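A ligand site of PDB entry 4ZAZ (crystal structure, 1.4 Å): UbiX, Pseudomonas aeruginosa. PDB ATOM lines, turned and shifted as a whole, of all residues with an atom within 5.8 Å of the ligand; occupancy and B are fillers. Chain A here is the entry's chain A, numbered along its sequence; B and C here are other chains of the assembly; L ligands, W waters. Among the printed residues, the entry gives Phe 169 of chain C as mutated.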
ATOM      1  N   MET A  11       9.005   0.587  -3.719  1.00  0.00           N
ATOM      2  CA  MET A  11       8.767  -0.255  -2.558  1.00  0.00           C
ATOM      3  C   MET A  11       9.811  -1.387  -2.543  1.00  0.00           C
ATOM      4  O   MET A  11       9.981  -2.097  -3.526  1.00  0.00           O
ATOM      5  CB  MET A  11       7.343  -0.852  -2.550  1.00  0.00           C
ATOM      6  CG  MET A  11       6.300   0.239  -2.487  1.00  0.00           C
ATOM      7  SD  MET A  11       4.613  -0.339  -2.260  1.00  0.00           S
ATOM      8  CE  MET A  11       4.726  -1.107  -0.644  1.00  0.00           C
ATOM      9  N   THR A  12      10.534  -1.495  -1.423  1.00  0.00           N
ATOM     10  CA  THR A  12      11.492  -2.561  -1.246  1.00  0.00           C
ATOM     11  C   THR A  12      11.127  -3.389  -0.011  1.00  0.00           C
ATOM     12  O   THR A  12      10.194  -3.035   0.715  1.00  0.00           O
ATOM     13  CB  THR A  12      12.949  -2.025  -1.203  1.00  0.00           C
ATOM     14  OG1 THR A  12      13.121  -1.231  -0.027  1.00  0.00           O
ATOM     15  CG2 THR A  12      13.214  -1.227  -2.464  1.00  0.00           C
ATOM     16  N   GLY A  13      11.861  -4.457   0.193  1.00  0.00           N
ATOM     17  CA  GLY A  13      11.462  -5.506   1.049  1.00  0.00           C
ATOM     18  C   GLY A  13      11.607  -5.396   2.550  1.00  0.00           C
ATOM     19  O   GLY A  13      11.943  -6.390   3.204  1.00  0.00           O
ATOM     20  N   ALA A  14      11.359  -4.230   3.116  1.00  0.00           N
ATOM     21  CA  ALA A  14      11.228  -4.092   4.554  1.00  0.00           C
ATOM     22  C   ALA A  14       9.754  -4.309   4.917  1.00  0.00           C
ATOM     23  O   ALA A  14       8.827  -4.058   4.117  1.00  0.00           O
ATOM     24  CB  ALA A  14      11.737  -2.749   5.047  1.00  0.00           C
ATOM     25  N   SER A  15       9.540  -4.740   6.128  1.00  0.00           N
ATOM     26  CA  SER A  15       8.221  -4.798   6.743  1.00  0.00           C
ATOM     27  C   SER A  15       7.617  -3.382   6.718  1.00  0.00           C
ATOM     28  O   SER A  15       8.327  -2.370   6.906  1.00  0.00           O
ATOM     29  CB  SER A  15       8.307  -5.353   8.168  1.00  0.00           C
ATOM     30  OG  SER A  15       6.992  -5.549   8.649  1.00  0.00           O
ATOM     31  N   SER A  39      10.432  -4.132  -5.664  1.00  0.00           N
ATOM     32  CA  SER A  39      11.357  -5.232  -5.697  1.00  0.00           C
ATOM     33  C   SER A  39      10.658  -6.593  -5.540  1.00  0.00           C
ATOM     34  O   SER A  39       9.535  -6.675  -5.051  1.00  0.00           O
ATOM     35  CB  SER A  39      12.385  -5.064  -4.595  1.00  0.00           C
ATOM     36  OG  SER A  39      11.863  -5.353  -3.331  1.00  0.00           O
ATOM     37  N   LYS A  40      11.362  -7.647  -5.939  1.00  0.00           N
ATOM     38  CA  LYS A  40      10.899  -9.021  -5.751  1.00  0.00           C
ATOM     39  C   LYS A  40      10.588  -9.269  -4.264  1.00  0.00           C
ATOM     40  O   LYS A  40       9.526  -9.817  -3.906  1.00  0.00           O
ATOM     41  CB  LYS A  40      11.961 -10.000  -6.276  1.00  0.00           C
ATOM     42  CG  LYS A  40      11.609 -11.469  -6.124  1.00  0.00           C
ATOM     43  CD  LYS A  40      12.780 -12.411  -6.410  1.00  0.00           C
ATOM     44  CE  LYS A  40      13.426 -12.135  -7.769  1.00  0.00           C
ATOM     45  NZ  LYS A  40      14.089 -13.342  -8.337  1.00  0.00           N
ATOM     46  N   ALA A  41      11.495  -8.872  -3.397  1.00  0.00           N
ATOM     47  CA  ALA A  41      11.293  -9.099  -1.977  1.00  0.00           C
ATOM     48  C   ALA A  41      10.072  -8.295  -1.481  1.00  0.00           C
ATOM     49  O   ALA A  41       9.305  -8.816  -0.631  1.00  0.00           O
ATOM     50  CB  ALA A  41      12.544  -8.784  -1.165  1.00  0.00           C
ATOM     51  N   ALA A  42       9.896  -7.072  -1.940  1.00  0.00           N
ATOM     52  CA  ALA A  42       8.721  -6.316  -1.567  1.00  0.00           C
ATOM     53  C   ALA A  42       7.420  -6.999  -1.984  1.00  0.00           C
ATOM     54  O   ALA A  42       6.421  -6.862  -1.285  1.00  0.00           O
ATOM     55  CB  ALA A  42       8.771  -4.919  -2.111  1.00  0.00           C
ATOM     56  N   LEU A  44       6.948 -10.153  -1.941  1.00  0.00           N
ATOM     57  CA  LEU A  44       6.722 -11.172  -0.919  1.00  0.00           C
ATOM     58  C   LEU A  44       6.294 -10.593   0.422  1.00  0.00           C
ATOM     59  O   LEU A  44       5.462 -11.202   1.112  1.00  0.00           O
ATOM     60  CB  LEU A  44       7.917 -12.078  -0.779  1.00  0.00           C
ATOM     61  CG  LEU A  44       7.767 -13.101   0.332  1.00  0.00           C
ATOM     62  CD1 LEU A  44       6.691 -14.154   0.060  1.00  0.00           C
ATOM     63  CD2 LEU A  44       9.147 -13.732   0.413  1.00  0.00           C
ATOM     64  N   VAL A  45       6.783  -9.391   0.765  1.00  0.00           N
ATOM     65  CA  VAL A  45       6.306  -8.701   1.950  1.00  0.00           C
ATOM     66  C   VAL A  45       4.814  -8.335   1.805  1.00  0.00           C
ATOM     67  O   VAL A  45       4.015  -8.542   2.737  1.00  0.00           O
ATOM     68  CB  VAL A  45       7.108  -7.436   2.266  1.00  0.00           C
ATOM     69  CG1 VAL A  45       6.468  -6.721   3.451  1.00  0.00           C
ATOM     70  CG2 VAL A  45       8.605  -7.744   2.537  1.00  0.00           C
ATOM     71  N   THR A  48       2.567 -11.249   2.320  1.00  0.00           N
ATOM     72  CA  THR A  48       2.638 -11.771   3.700  1.00  0.00           C
ATOM     73  C   THR A  48       1.831 -10.848   4.655  1.00  0.00           C
ATOM     74  O   THR A  48       1.163 -11.362   5.549  1.00  0.00           O
ATOM     75  CB  THR A  48       4.138 -11.777   4.127  1.00  0.00           C
ATOM     76  OG1 THR A  48       4.849 -12.680   3.261  1.00  0.00           O
ATOM     77  CG2 THR A  48       4.294 -12.217   5.581  1.00  0.00           C
ATOM     78  N   GLU A  49       1.888  -9.522   4.460  1.00  0.00           N
ATOM     79  CA  GLU A  49       1.412  -8.547   5.415  1.00  0.00           C
ATOM     80  C   GLU A  49       0.117  -7.949   5.083  1.00  0.00           C
ATOM     81  O   GLU A  49      -0.458  -7.315   5.945  1.00  0.00           O
ATOM     82  CB  GLU A  49       2.364  -7.338   5.527  1.00  0.00           C
ATOM     83  CG  GLU A  49       3.671  -7.773   5.993  1.00  0.00           C
ATOM     84  CD  GLU A  49       4.578  -6.603   6.435  1.00  0.00           C
ATOM     85  OE1 GLU A  49       4.422  -5.392   6.023  1.00  0.00           O
ATOM     86  OE2 GLU A  49       5.539  -6.969   7.138  1.00  0.00           O
ATOM     87  N   CYS A 103      12.040   1.070   2.850  1.00  0.00           N
ATOM     88  CA  CYS A 103      13.416   0.928   2.371  1.00  0.00           C
ATOM     89  C   CYS A 103      14.080  -0.199   3.194  1.00  0.00           C
ATOM     90  O   CYS A 103      14.344  -0.004   4.376  1.00  0.00           O
ATOM     91  CB  CYS A 103      14.211   2.220   2.537  1.00  0.00           C
ATOM     92  SG  CYS A 103      15.831   2.113   1.797  1.00  0.00           S
ATOM     93  N   SER A 104      14.350  -1.331   2.556  1.00  0.00           N
ATOM     94  CA  SER A 104      15.077  -2.393   3.210  1.00  0.00           C
ATOM     95  C   SER A 104      16.528  -1.946   3.551  1.00  0.00           C
ATOM     96  O   SER A 104      17.081  -1.029   2.954  1.00  0.00           O
ATOM     97  CB  SER A 104      15.176  -3.606   2.329  1.00  0.00           C
ATOM     98  OG  SER A 104      16.032  -3.346   1.240  1.00  0.00           O
ATOM     99  N   THR A 105      17.133  -2.668   4.498  1.00  0.00           N
ATOM    100  CA  THR A 105      18.530  -2.405   4.813  1.00  0.00           C
ATOM    101  C   THR A 105      19.407  -2.669   3.575  1.00  0.00           C
ATOM    102  O   THR A 105      20.408  -1.989   3.371  1.00  0.00           O
ATOM    103  CB  THR A 105      19.028  -3.145   6.052  1.00  0.00           C
ATOM    104  OG1 THR A 105      18.965  -4.543   5.814  1.00  0.00           O
ATOM    105  CG2 THR A 105      18.252  -2.794   7.270  1.00  0.00           C
ATOM    106  N   GLY A 106      19.044  -3.653   2.761  1.00  0.00           N
ATOM    107  CA  GLY A 106      19.826  -3.932   1.558  1.00  0.00           C
ATOM    108  C   GLY A 106      19.738  -2.835   0.504  1.00  0.00           C
ATOM    109  O   GLY A 106      20.732  -2.535  -0.148  1.00  0.00           O
ATOM    110  N   THR A 107      18.535  -2.257   0.337  1.00  0.00           N
ATOM    111  CA  THR A 107      18.417  -1.130  -0.587  1.00  0.00           C
ATOM    112  C   THR A 107      19.128   0.114  -0.014  1.00  0.00           C
ATOM    113  O   THR A 107      19.813   0.821  -0.763  1.00  0.00           O
ATOM    114  CB  THR A 107      16.967  -0.896  -1.015  1.00  0.00           C
ATOM    115  OG1 THR A 107      16.524  -1.997  -1.856  1.00  0.00           O
ATOM    116  CG2 THR A 107      16.851   0.417  -1.762  1.00  0.00           C
ATOM    117  N   ASN A 118      19.609  -2.669  -9.931  1.00  0.00           N
ATOM    118  CA  ASN A 118      18.280  -2.689 -10.512  1.00  0.00           C
ATOM    119  C   ASN A 118      17.790  -1.255 -10.647  1.00  0.00           C
ATOM    120  O   ASN A 118      18.502  -0.282 -10.300  1.00  0.00           O
ATOM    121  CB  ASN A 118      17.350  -3.489  -9.608  1.00  0.00           C
ATOM    122  CG  ASN A 118      17.329  -2.954  -8.186  1.00  0.00           C
ATOM    123  OD1 ASN A 118      17.137  -1.805  -7.967  1.00  0.00           O
ATOM    124  ND2 ASN A 118      17.456  -3.836  -7.222  1.00  0.00           N
ATOM    125  N   GLU A 121      17.665   1.050  -7.484  1.00  0.00           N
ATOM    126  CA  GLU A 121      18.987   1.554  -7.004  1.00  0.00           C
ATOM    127  C   GLU A 121      19.596   2.561  -7.990  1.00  0.00           C
ATOM    128  O   GLU A 121      20.137   3.592  -7.579  1.00  0.00           O
ATOM    129  CB  GLU A 121      19.911   0.326  -6.834  1.00  0.00           C
ATOM    130  CG  GLU A 121      19.437  -0.586  -5.700  1.00  0.00           C
ATOM    131  CD  GLU A 121      20.105  -1.924  -5.609  1.00  0.00           C
ATOM    132  OE1 GLU A 121      21.151  -2.123  -6.300  1.00  0.00           O
ATOM    133  OE2 GLU A 121      19.588  -2.802  -4.841  1.00  0.00           O
ATOM    134  N   ARG A 139      12.790   0.571   7.779  1.00  0.00           N
ATOM    135  CA  ARG A 139      12.047  -0.067   8.880  1.00  0.00           C
ATOM    136  C   ARG A 139      12.903  -1.246   9.370  1.00  0.00           C
ATOM    137  O   ARG A 139      13.076  -2.236   8.659  1.00  0.00           O
ATOM    138  CB  ARG A 139      10.679  -0.560   8.388  1.00  0.00           C
ATOM    139  CG  ARG A 139       9.644  -0.867   9.453  1.00  0.00           C
ATOM    140  CD  ARG A 139      10.121  -1.611  10.685  1.00  0.00           C
ATOM    141  NE  ARG A 139      10.578  -2.951  10.405  1.00  0.00           N
ATOM    142  CZ  ARG A 139      11.104  -3.766  11.297  1.00  0.00           C
ATOM    143  NH1 ARG A 139      11.130  -3.429  12.572  1.00  0.00           N
ATOM    144  NH2 ARG A 139      11.606  -4.886  10.906  1.00  0.00           N
ATOM    145  N   GLU A 140      13.575  -1.047  10.504  1.00  0.00           N
ATOM    146  CA  GLU A 140      14.459  -2.068  11.023  1.00  0.00           C
ATOM    147  C   GLU A 140      14.638  -1.689  12.490  1.00  0.00           C
ATOM    148  O   GLU A 140      14.555  -0.538  12.884  1.00  0.00           O
ATOM    149  CB  GLU A 140      15.792  -2.165  10.261  1.00  0.00           C
ATOM    150  CG  GLU A 140      16.718  -3.288  10.683  1.00  0.00           C
ATOM    151  CD  GLU A 140      16.055  -4.643  10.602  1.00  0.00           C
ATOM    152  OE1 GLU A 140      15.347  -5.032  11.574  1.00  0.00           O
ATOM    153  OE2 GLU A 140      16.294  -5.347   9.607  1.00  0.00           O
ATOM    154  N   TRP B  84      13.256 -16.131   2.919  1.00  0.00           N
ATOM    155  CA  TRP B  84      13.117 -15.155   3.979  1.00  0.00           C
ATOM    156  C   TRP B  84      12.250 -15.656   5.163  1.00  0.00           C
ATOM    157  O   TRP B  84      12.182 -15.024   6.214  1.00  0.00           O
ATOM    158  CB  TRP B  84      12.528 -13.827   3.426  1.00  0.00           C
ATOM    159  CG  TRP B  84      13.289 -13.336   2.208  1.00  0.00           C
ATOM    160  CD1 TRP B  84      12.814 -13.252   0.973  1.00  0.00           C
ATOM    161  CD2 TRP B  84      14.682 -13.013   2.102  1.00  0.00           C
ATOM    162  NE1 TRP B  84      13.770 -12.832   0.113  1.00  0.00           N
ATOM    163  CE2 TRP B  84      14.943 -12.722   0.769  1.00  0.00           C
ATOM    164  CE3 TRP B  84      15.742 -12.928   3.008  1.00  0.00           C
ATOM    165  CZ2 TRP B  84      16.187 -12.348   0.305  1.00  0.00           C
ATOM    166  CZ3 TRP B  84      17.003 -12.572   2.560  1.00  0.00           C
ATOM    167  CH2 TRP B  84      17.216 -12.260   1.217  1.00  0.00           C
ATOM    168  N   MET B  85      11.540 -16.751   4.978  1.00  0.00           N
ATOM    169  CA  MET B  85      10.790 -17.368   6.061  1.00  0.00           C
ATOM    170  C   MET B  85      11.630 -18.220   6.978  1.00  0.00           C
ATOM    171  O   MET B  85      11.135 -18.680   8.001  1.00  0.00           O
ATOM    172  CB  MET B  85       9.650 -18.246   5.500  1.00  0.00           C
ATOM    173  CG  MET B  85       8.601 -17.502   4.751  1.00  0.00           C
ATOM    174  SD  MET B  85       8.336 -15.755   4.747  1.00  0.00           S
ATOM    175  CE  MET B  85       8.847 -15.159   3.143  1.00  0.00           C
ATOM    176  N   ALA B  86      12.919 -18.361   6.678  1.00  0.00           N
ATOM    177  CA  ALA B  86      13.795 -19.128   7.555  1.00  0.00           C
ATOM    178  C   ALA B  86      14.230 -18.281   8.773  1.00  0.00           C
ATOM    179  O   ALA B  86      14.362 -17.041   8.660  1.00  0.00           O
ATOM    180  CB  ALA B  86      14.983 -19.534   6.782  1.00  0.00           C
ATOM    181  N   ALA B  89      16.754 -15.018   8.871  1.00  0.00           N
ATOM    182  CA  ALA B  89      16.396 -13.777   8.190  1.00  0.00           C
ATOM    183  C   ALA B  89      15.876 -12.643   9.114  1.00  0.00           C
ATOM    184  O   ALA B  89      15.813 -11.481   8.682  1.00  0.00           O
ATOM    185  CB  ALA B  89      15.361 -14.057   7.141  1.00  0.00           C
ATOM    186  N   SER B  90      15.444 -12.997  10.318  1.00  0.00           N
ATOM    187  CA  SER B  90      14.872 -12.054  11.276  1.00  0.00           C
ATOM    188  C   SER B  90      15.586 -12.127  12.605  1.00  0.00           C
ATOM    189  O   SER B  90      15.892 -13.205  13.125  1.00  0.00           O
ATOM    190  CB  SER B  90      13.377 -12.326  11.547  1.00  0.00           C
ATOM    191  OG  SER B  90      12.906 -11.477  12.613  1.00  0.00           O
ATOM    192  N   ALA B 115      24.890  -5.299   2.227  1.00  0.00           N
ATOM    193  CA  ALA B 115      24.137  -5.567   0.999  1.00  0.00           C
ATOM    194  C   ALA B 115      22.875  -6.494   1.146  1.00  0.00           C
ATOM    195  O   ALA B 115      21.921  -6.317   0.396  1.00  0.00           O
ATOM    196  CB  ALA B 115      25.068  -6.044  -0.083  1.00  0.00           C
ATOM    197  N   CYS B 116      22.893  -7.452   2.020  1.00  0.00           N
ATOM    198  CA  CYS B 116      21.684  -8.312   2.214  1.00  0.00           C
ATOM    199  C   CYS B 116      21.018  -8.851   0.918  1.00  0.00           C
ATOM    200  O   CYS B 116      19.793  -8.997   0.900  1.00  0.00           O
ATOM    201  CB  CYS B 116      20.623  -7.551   3.016  1.00  0.00           C
ATOM    202  SG  CYS B 116      20.941  -7.154   4.674  1.00  0.00           S
ATOM    203  N   ASN B 117      21.812  -9.275  -0.085  1.00  0.00           N
ATOM    204  CA  ASN B 117      21.255  -9.788  -1.306  1.00  0.00           C
ATOM    205  C   ASN B 117      20.771 -11.247  -1.396  1.00  0.00           C
ATOM    206  O   ASN B 117      20.070 -11.622  -2.316  1.00  0.00           O
ATOM    207  CB  ASN B 117      22.159  -9.519  -2.474  1.00  0.00           C
ATOM    208  CG  ASN B 117      22.142  -8.018  -2.886  1.00  0.00           C
ATOM    209  OD1 ASN B 117      21.075  -7.399  -2.980  1.00  0.00           O
ATOM    210  ND2 ASN B 117      23.314  -7.478  -3.151  1.00  0.00           N
ATOM    211  N   ASN B 118      21.078 -11.999  -0.411  1.00  0.00           N
ATOM    212  CA  ASN B 118      20.610 -13.361  -0.241  1.00  0.00           C
ATOM    213  C   ASN B 118      20.564 -13.674   1.247  1.00  0.00           C
ATOM    214  O   ASN B 118      20.882 -12.820   2.108  1.00  0.00           O
ATOM    215  CB  ASN B 118      21.563 -14.311  -0.959  1.00  0.00           C
ATOM    216  CG  ASN B 118      22.998 -14.151  -0.486  1.00  0.00           C
ATOM    217  OD1 ASN B 118      23.270 -14.178   0.667  1.00  0.00           O
ATOM    218  ND2 ASN B 118      23.918 -14.061  -1.417  1.00  0.00           N
ATOM    219  N   ARG B 122      21.887 -11.517   4.540  1.00  0.00           N
ATOM    220  CA  ARG B 122      20.900 -11.025   5.480  1.00  0.00           C
ATOM    221  C   ARG B 122      21.104 -11.596   6.833  1.00  0.00           C
ATOM    222  O   ARG B 122      20.963 -10.927   7.868  1.00  0.00           O
ATOM    223  CB  ARG B 122      19.485 -11.339   4.960  1.00  0.00           C
ATOM    224  CG  ARG B 122      18.363 -11.003   5.920  1.00  0.00           C
ATOM    225  CD  ARG B 122      18.222  -9.542   6.289  1.00  0.00           C
ATOM    226  NE  ARG B 122      17.088  -9.399   7.205  1.00  0.00           N
ATOM    227  CZ  ARG B 122      16.806  -8.278   7.823  1.00  0.00           C
ATOM    228  NH1 ARG B 122      17.461  -7.126   7.523  1.00  0.00           N
ATOM    229  NH2 ARG B 122      15.849  -8.271   8.738  1.00  0.00           N
ATOM    230  N   PHE C 169       4.925  -7.709  10.264  1.00  0.00           N
ATOM    231  CA  PHE C 169       4.960  -9.065   9.769  1.00  0.00           C
ATOM    232  C   PHE C 169       4.204 -10.083  10.657  1.00  0.00           C
ATOM    233  O   PHE C 169       4.039 -11.247  10.252  1.00  0.00           O
ATOM    234  CB  PHE C 169       6.367  -9.515   9.423  1.00  0.00           C
ATOM    235  CG  PHE C 169       7.377  -9.435  10.541  1.00  0.00           C
ATOM    236  CD1 PHE C 169       7.505 -10.418  11.486  1.00  0.00           C
ATOM    237  CD2 PHE C 169       8.259  -8.358  10.593  1.00  0.00           C
ATOM    238  CE1 PHE C 169       8.504 -10.402  12.428  1.00  0.00           C
ATOM    239  CE2 PHE C 169       9.241  -8.298  11.562  1.00  0.00           C
ATOM    240  CZ  PHE C 169       9.383  -9.332  12.449  1.00  0.00           C
ATOM    241  N   TRP C 200      10.676 -16.118  14.915  1.00  0.00           N
ATOM    242  CA  TRP C 200      10.529 -16.258  13.493  1.00  0.00           C
ATOM    243  C   TRP C 200      11.084 -17.541  12.917  1.00  0.00           C
ATOM    244  O   TRP C 200      12.247 -17.867  13.151  1.00  0.00           O
ATOM    245  CB  TRP C 200      11.247 -15.097  12.797  1.00  0.00           C
ATOM    246  CG  TRP C 200      11.046 -15.055  11.308  1.00  0.00           C
ATOM    247  CD1 TRP C 200      11.942 -15.408  10.333  1.00  0.00           C
ATOM    248  CD2 TRP C 200       9.865 -14.653  10.584  1.00  0.00           C
ATOM    249  NE1 TRP C 200      11.409 -15.254   9.093  1.00  0.00           N
ATOM    250  CE2 TRP C 200      10.130 -14.781   9.226  1.00  0.00           C
ATOM    251  CE3 TRP C 200       8.631 -14.169  10.965  1.00  0.00           C
ATOM    252  CZ2 TRP C 200       9.218 -14.436   8.269  1.00  0.00           C
ATOM    253  CZ3 TRP C 200       7.694 -13.867   9.978  1.00  0.00           C
ATOM    254  CH2 TRP C 200       7.987 -14.036   8.673  1.00  0.00           C
HETATM  255  C1  LIG L   1      12.400  -6.777   6.830  1.00  0.00           C
HETATM  256  C2  LIG L   1      10.355 -11.121   8.972  1.00  0.00           C
HETATM  257  C3  LIG L   1       9.915 -11.431   3.282  1.00  0.00           C
HETATM  258  C4  LIG L   1       7.961 -10.654   5.376  1.00  0.00           C
HETATM  259  O1  LIG L   1      16.035  -4.464  -1.031  1.00  0.00           O
HETATM  260  P1  LIG L   1      15.216  -5.584  -1.637  1.00  0.00           P
HETATM  261  O2  LIG L   1      15.595  -5.827  -3.115  1.00  0.00           O
HETATM  262  O3  LIG L   1      13.737  -5.427  -1.476  1.00  0.00           O
HETATM  263  O4  LIG L   1      15.707  -6.922  -0.925  1.00  0.00           O
HETATM  264  C5  LIG L   1      15.540  -7.079   0.495  1.00  0.00           C
HETATM  265  C6  LIG L   1      15.889  -8.503   0.887  1.00  0.00           C
HETATM  266  O5  LIG L   1      17.072  -8.943   0.305  1.00  0.00           O
HETATM  267  C7  LIG L   1      15.687  -8.812   2.310  1.00  0.00           C
HETATM  268  O6  LIG L   1      16.916  -8.537   2.980  1.00  0.00           O
HETATM  269  C8  LIG L   1      14.471  -8.424   3.006  1.00  0.00           C
HETATM  270  O7  LIG L   1      13.366  -8.405   2.177  1.00  0.00           O
HETATM  271  C9  LIG L   1      14.291  -8.863   4.435  1.00  0.00           C
HETATM  272  N1  LIG L   1      13.196  -8.324   5.214  1.00  0.00           N
HETATM  273  C10 LIG L   1      11.935  -8.931   5.183  1.00  0.00           C
HETATM  274  C11 LIG L   1      11.536  -9.878   4.256  1.00  0.00           C
HETATM  275  C12 LIG L   1      10.249 -10.468   4.292  1.00  0.00           C
HETATM  276  C13 LIG L   1       9.320 -10.051   5.288  1.00  0.00           C
HETATM  277  C14 LIG L   1       9.733  -9.065   6.165  1.00  0.00           C
HETATM  278  C15 LIG L   1      11.007  -8.541   6.145  1.00  0.00           C
HETATM  279  N2  LIG L   1      11.319  -7.640   7.114  1.00  0.00           N
HETATM  280  C16 LIG L   1      11.471  -8.236   8.494  1.00  0.00           C
HETATM  281  C17 LIG L   1      12.285  -9.529   8.310  1.00  0.00           C
HETATM  282  C18 LIG L   1      11.685 -10.828   8.396  1.00  0.00           C
HETATM  283  C19 LIG L   1      12.489 -11.964   7.840  1.00  0.00           C
HETATM  284  C20 LIG L   1      13.344  -7.185   5.883  1.00  0.00           C
HETATM  285  N3  LIG L   1      14.423  -6.346   5.618  1.00  0.00           N
HETATM  286  C21 LIG L   1      14.533  -5.142   6.279  1.00  0.00           C
HETATM  287  O8  LIG L   1      15.499  -4.375   5.976  1.00  0.00           O
HETATM  288  N4  LIG L   1      13.579  -4.797   7.130  1.00  0.00           N
HETATM  289  C22 LIG L   1      12.515  -5.536   7.442  1.00  0.00           C
HETATM  290  O9  LIG L   1      11.628  -5.060   8.191  1.00  0.00           O
HETATM  291  O   HOH W   1      18.676  -4.213  -2.433  1.00  0.00           O
HETATM  292  O   HOH W   2      15.955  -3.335  -4.557  1.00  0.00           O
HETATM  293  O   HOH W   3      17.926  -7.260  -3.525  1.00  0.00           O
HETATM  294  O   HOH W   4      17.577  -9.810  -2.101  1.00  0.00           O
HETATM  295  O   HOH W   5      14.280  -8.015  -4.173  1.00  0.00           O
HETATM  296  O   HOH W   6      18.766  -6.368  -0.561  1.00  0.00           O
HETATM  297  O   HOH W   7      14.955  -1.107   6.695  1.00  0.00           O
HETATM  298  O   HOH W   8      17.171  -5.981   4.075  1.00  0.00           O
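Water W4 lies within hydrogen-bond range of O5 of the ligand (2.6 Å) and O of Asn 117 of chain B (3.1 Å).
Water W5 lies within hydrogen-bond range of an oxygen (O2) of the ligand, the backbone NH of Ala 41 and the backbone NH of Lys 40.
Water W3 bridges O2 of the ligand and OD1 of Asn 117 of chain B.
Water W8 lies within hydrogen-bond range of O6 of the ligand (2.8 Å), OG1 of Thr 105 (2.9 Å) and N of Gly 106 (3.3 Å).
Water W2 lies within hydrogen-bond range of O2 of the ligand, OG1 of Thr 107 and ND2 of Asn 118 of chain A.
Water W1 lies within hydrogen-bond range of OE2 of Glu 121, O1 of the ligand and OG1 of Thr 107.
OG of Ser 15 lies within hydrogen-bond range of N of Phe 169 of chain C (3.4 Å).
The backbone NH (N) of Ser 104 is in hydrogen-bond range of the side-chain hydroxyl (OG1) of Thr 12, at 2.9 Å.
OG of Ser 15 is in hydrogen-bond range of OE2 of Glu 49 (2.5 Å).
OG1 of Thr 105 is in hydrogen-bond range of NH1 of Arg 122 of chain B (3.4 Å).
The guanidinium group (NH2) of Arg 139 lies within salt-bridge range of the side-chain carboxylate (OE1) of Glu 140, 3.8 Å away.
O of Ala 89 of chain B is in hydrogen-bond range of NE of Arg 122 of chain B (2.9 Å).
The side-chain carboxylate (OE2) of Glu 140 lies within salt-bridge range of the guanidinium group (NH1) of Arg 122 of chain B (3.0 Å).
O of Leu 44 sits at hydrogen-bond distance from OG1 of Thr 48 (2.7 Å).
CB of Thr 12 touches O3 of the ligand, at 3.5 Å.
Ala 14 touches the ligand.
Ala 41 touches the ligand (CB to O7, 3.5 Å).
Leu 44 touches the ligand (CD2 to C3, 3.8 Å).
CG2 of Val 45 touches C12 of the ligand, 3.6 Å away.
CG2 of Thr 48 touches C4 of the ligand (3.99 Å).
Glu 140 touches the ligand.
Trp 84 of chain B touches the ligand.
CE of Met 85 of chain B touches C3 of the ligand (3.9 Å).
O of Ala 89 of chain B touches C19 of the ligand, at 3.5 Å.
Ser 90 of chain B touches the ligand.
NH1 of Arg 122 of chain B touches N3 of the ligand, 3.7 Å away.
Phe 169 of chain C touches the ligand.
Trp 200 of chain C touches the ligand.
22 residues have an atom within 4 Å of the ligand: Thr 12, Gly 13, Ala 14, Ser 15, Ser 39, Ala 41, Leu 44, Val 45, Thr 48, Ser 104, Thr 105, Thr 107, Arg 139, Glu 140, Trp 84 of chain B, Met 85 of chain B, Ala 89 of chain B, Ser 90 of chain B, Cys 116 of chain B, Arg 122 of chain B, Phe 169 of chain C and Trp 200 of chain C.
Along chain A the residues within 4 Å of the ligand span positions 12 to 140.
The side-chain hydroxyl (OG1) of Thr 107 is in hydrogen-bond range of an oxygen (O1) of the ligand.
The side-chain hydroxyl (OG) of Ser 39 sits at hydrogen-bond distance from an oxygen (O3) of the ligand (2.6 Å).
N of Ser 15 lies within hydrogen-bond range of O9 of the ligand (3.0 Å).
O of Gly 13 lies within hydrogen-bond range of O7 of the ligand (2.7 Å).
The side-chain hydroxyl (OG) of Ser 104 is in hydrogen-bond range of an oxygen (O1) of the ligand (2.5 Å).
O of Cys 116 of chain B lies within hydrogen-bond range of O5 of the ligand.
N of Gly 13 sits at hydrogen-bond distance from O3 of the ligand (2.7 Å).
A nitrogen (N4) of the ligand lies within hydrogen-bond range of the backbone carbonyl oxygen (O) of Arg 139, at 3.0 Å.
An oxygen (O9) of the ligand sits at hydrogen-bond distance from the guanidinium group of Arg 139 (2.7 Å).
N of Thr 105 is in hydrogen-bond range of O8 of the ligand.
OG1 of Thr 105 lies close to O8 of the ligand (3.5 Å).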
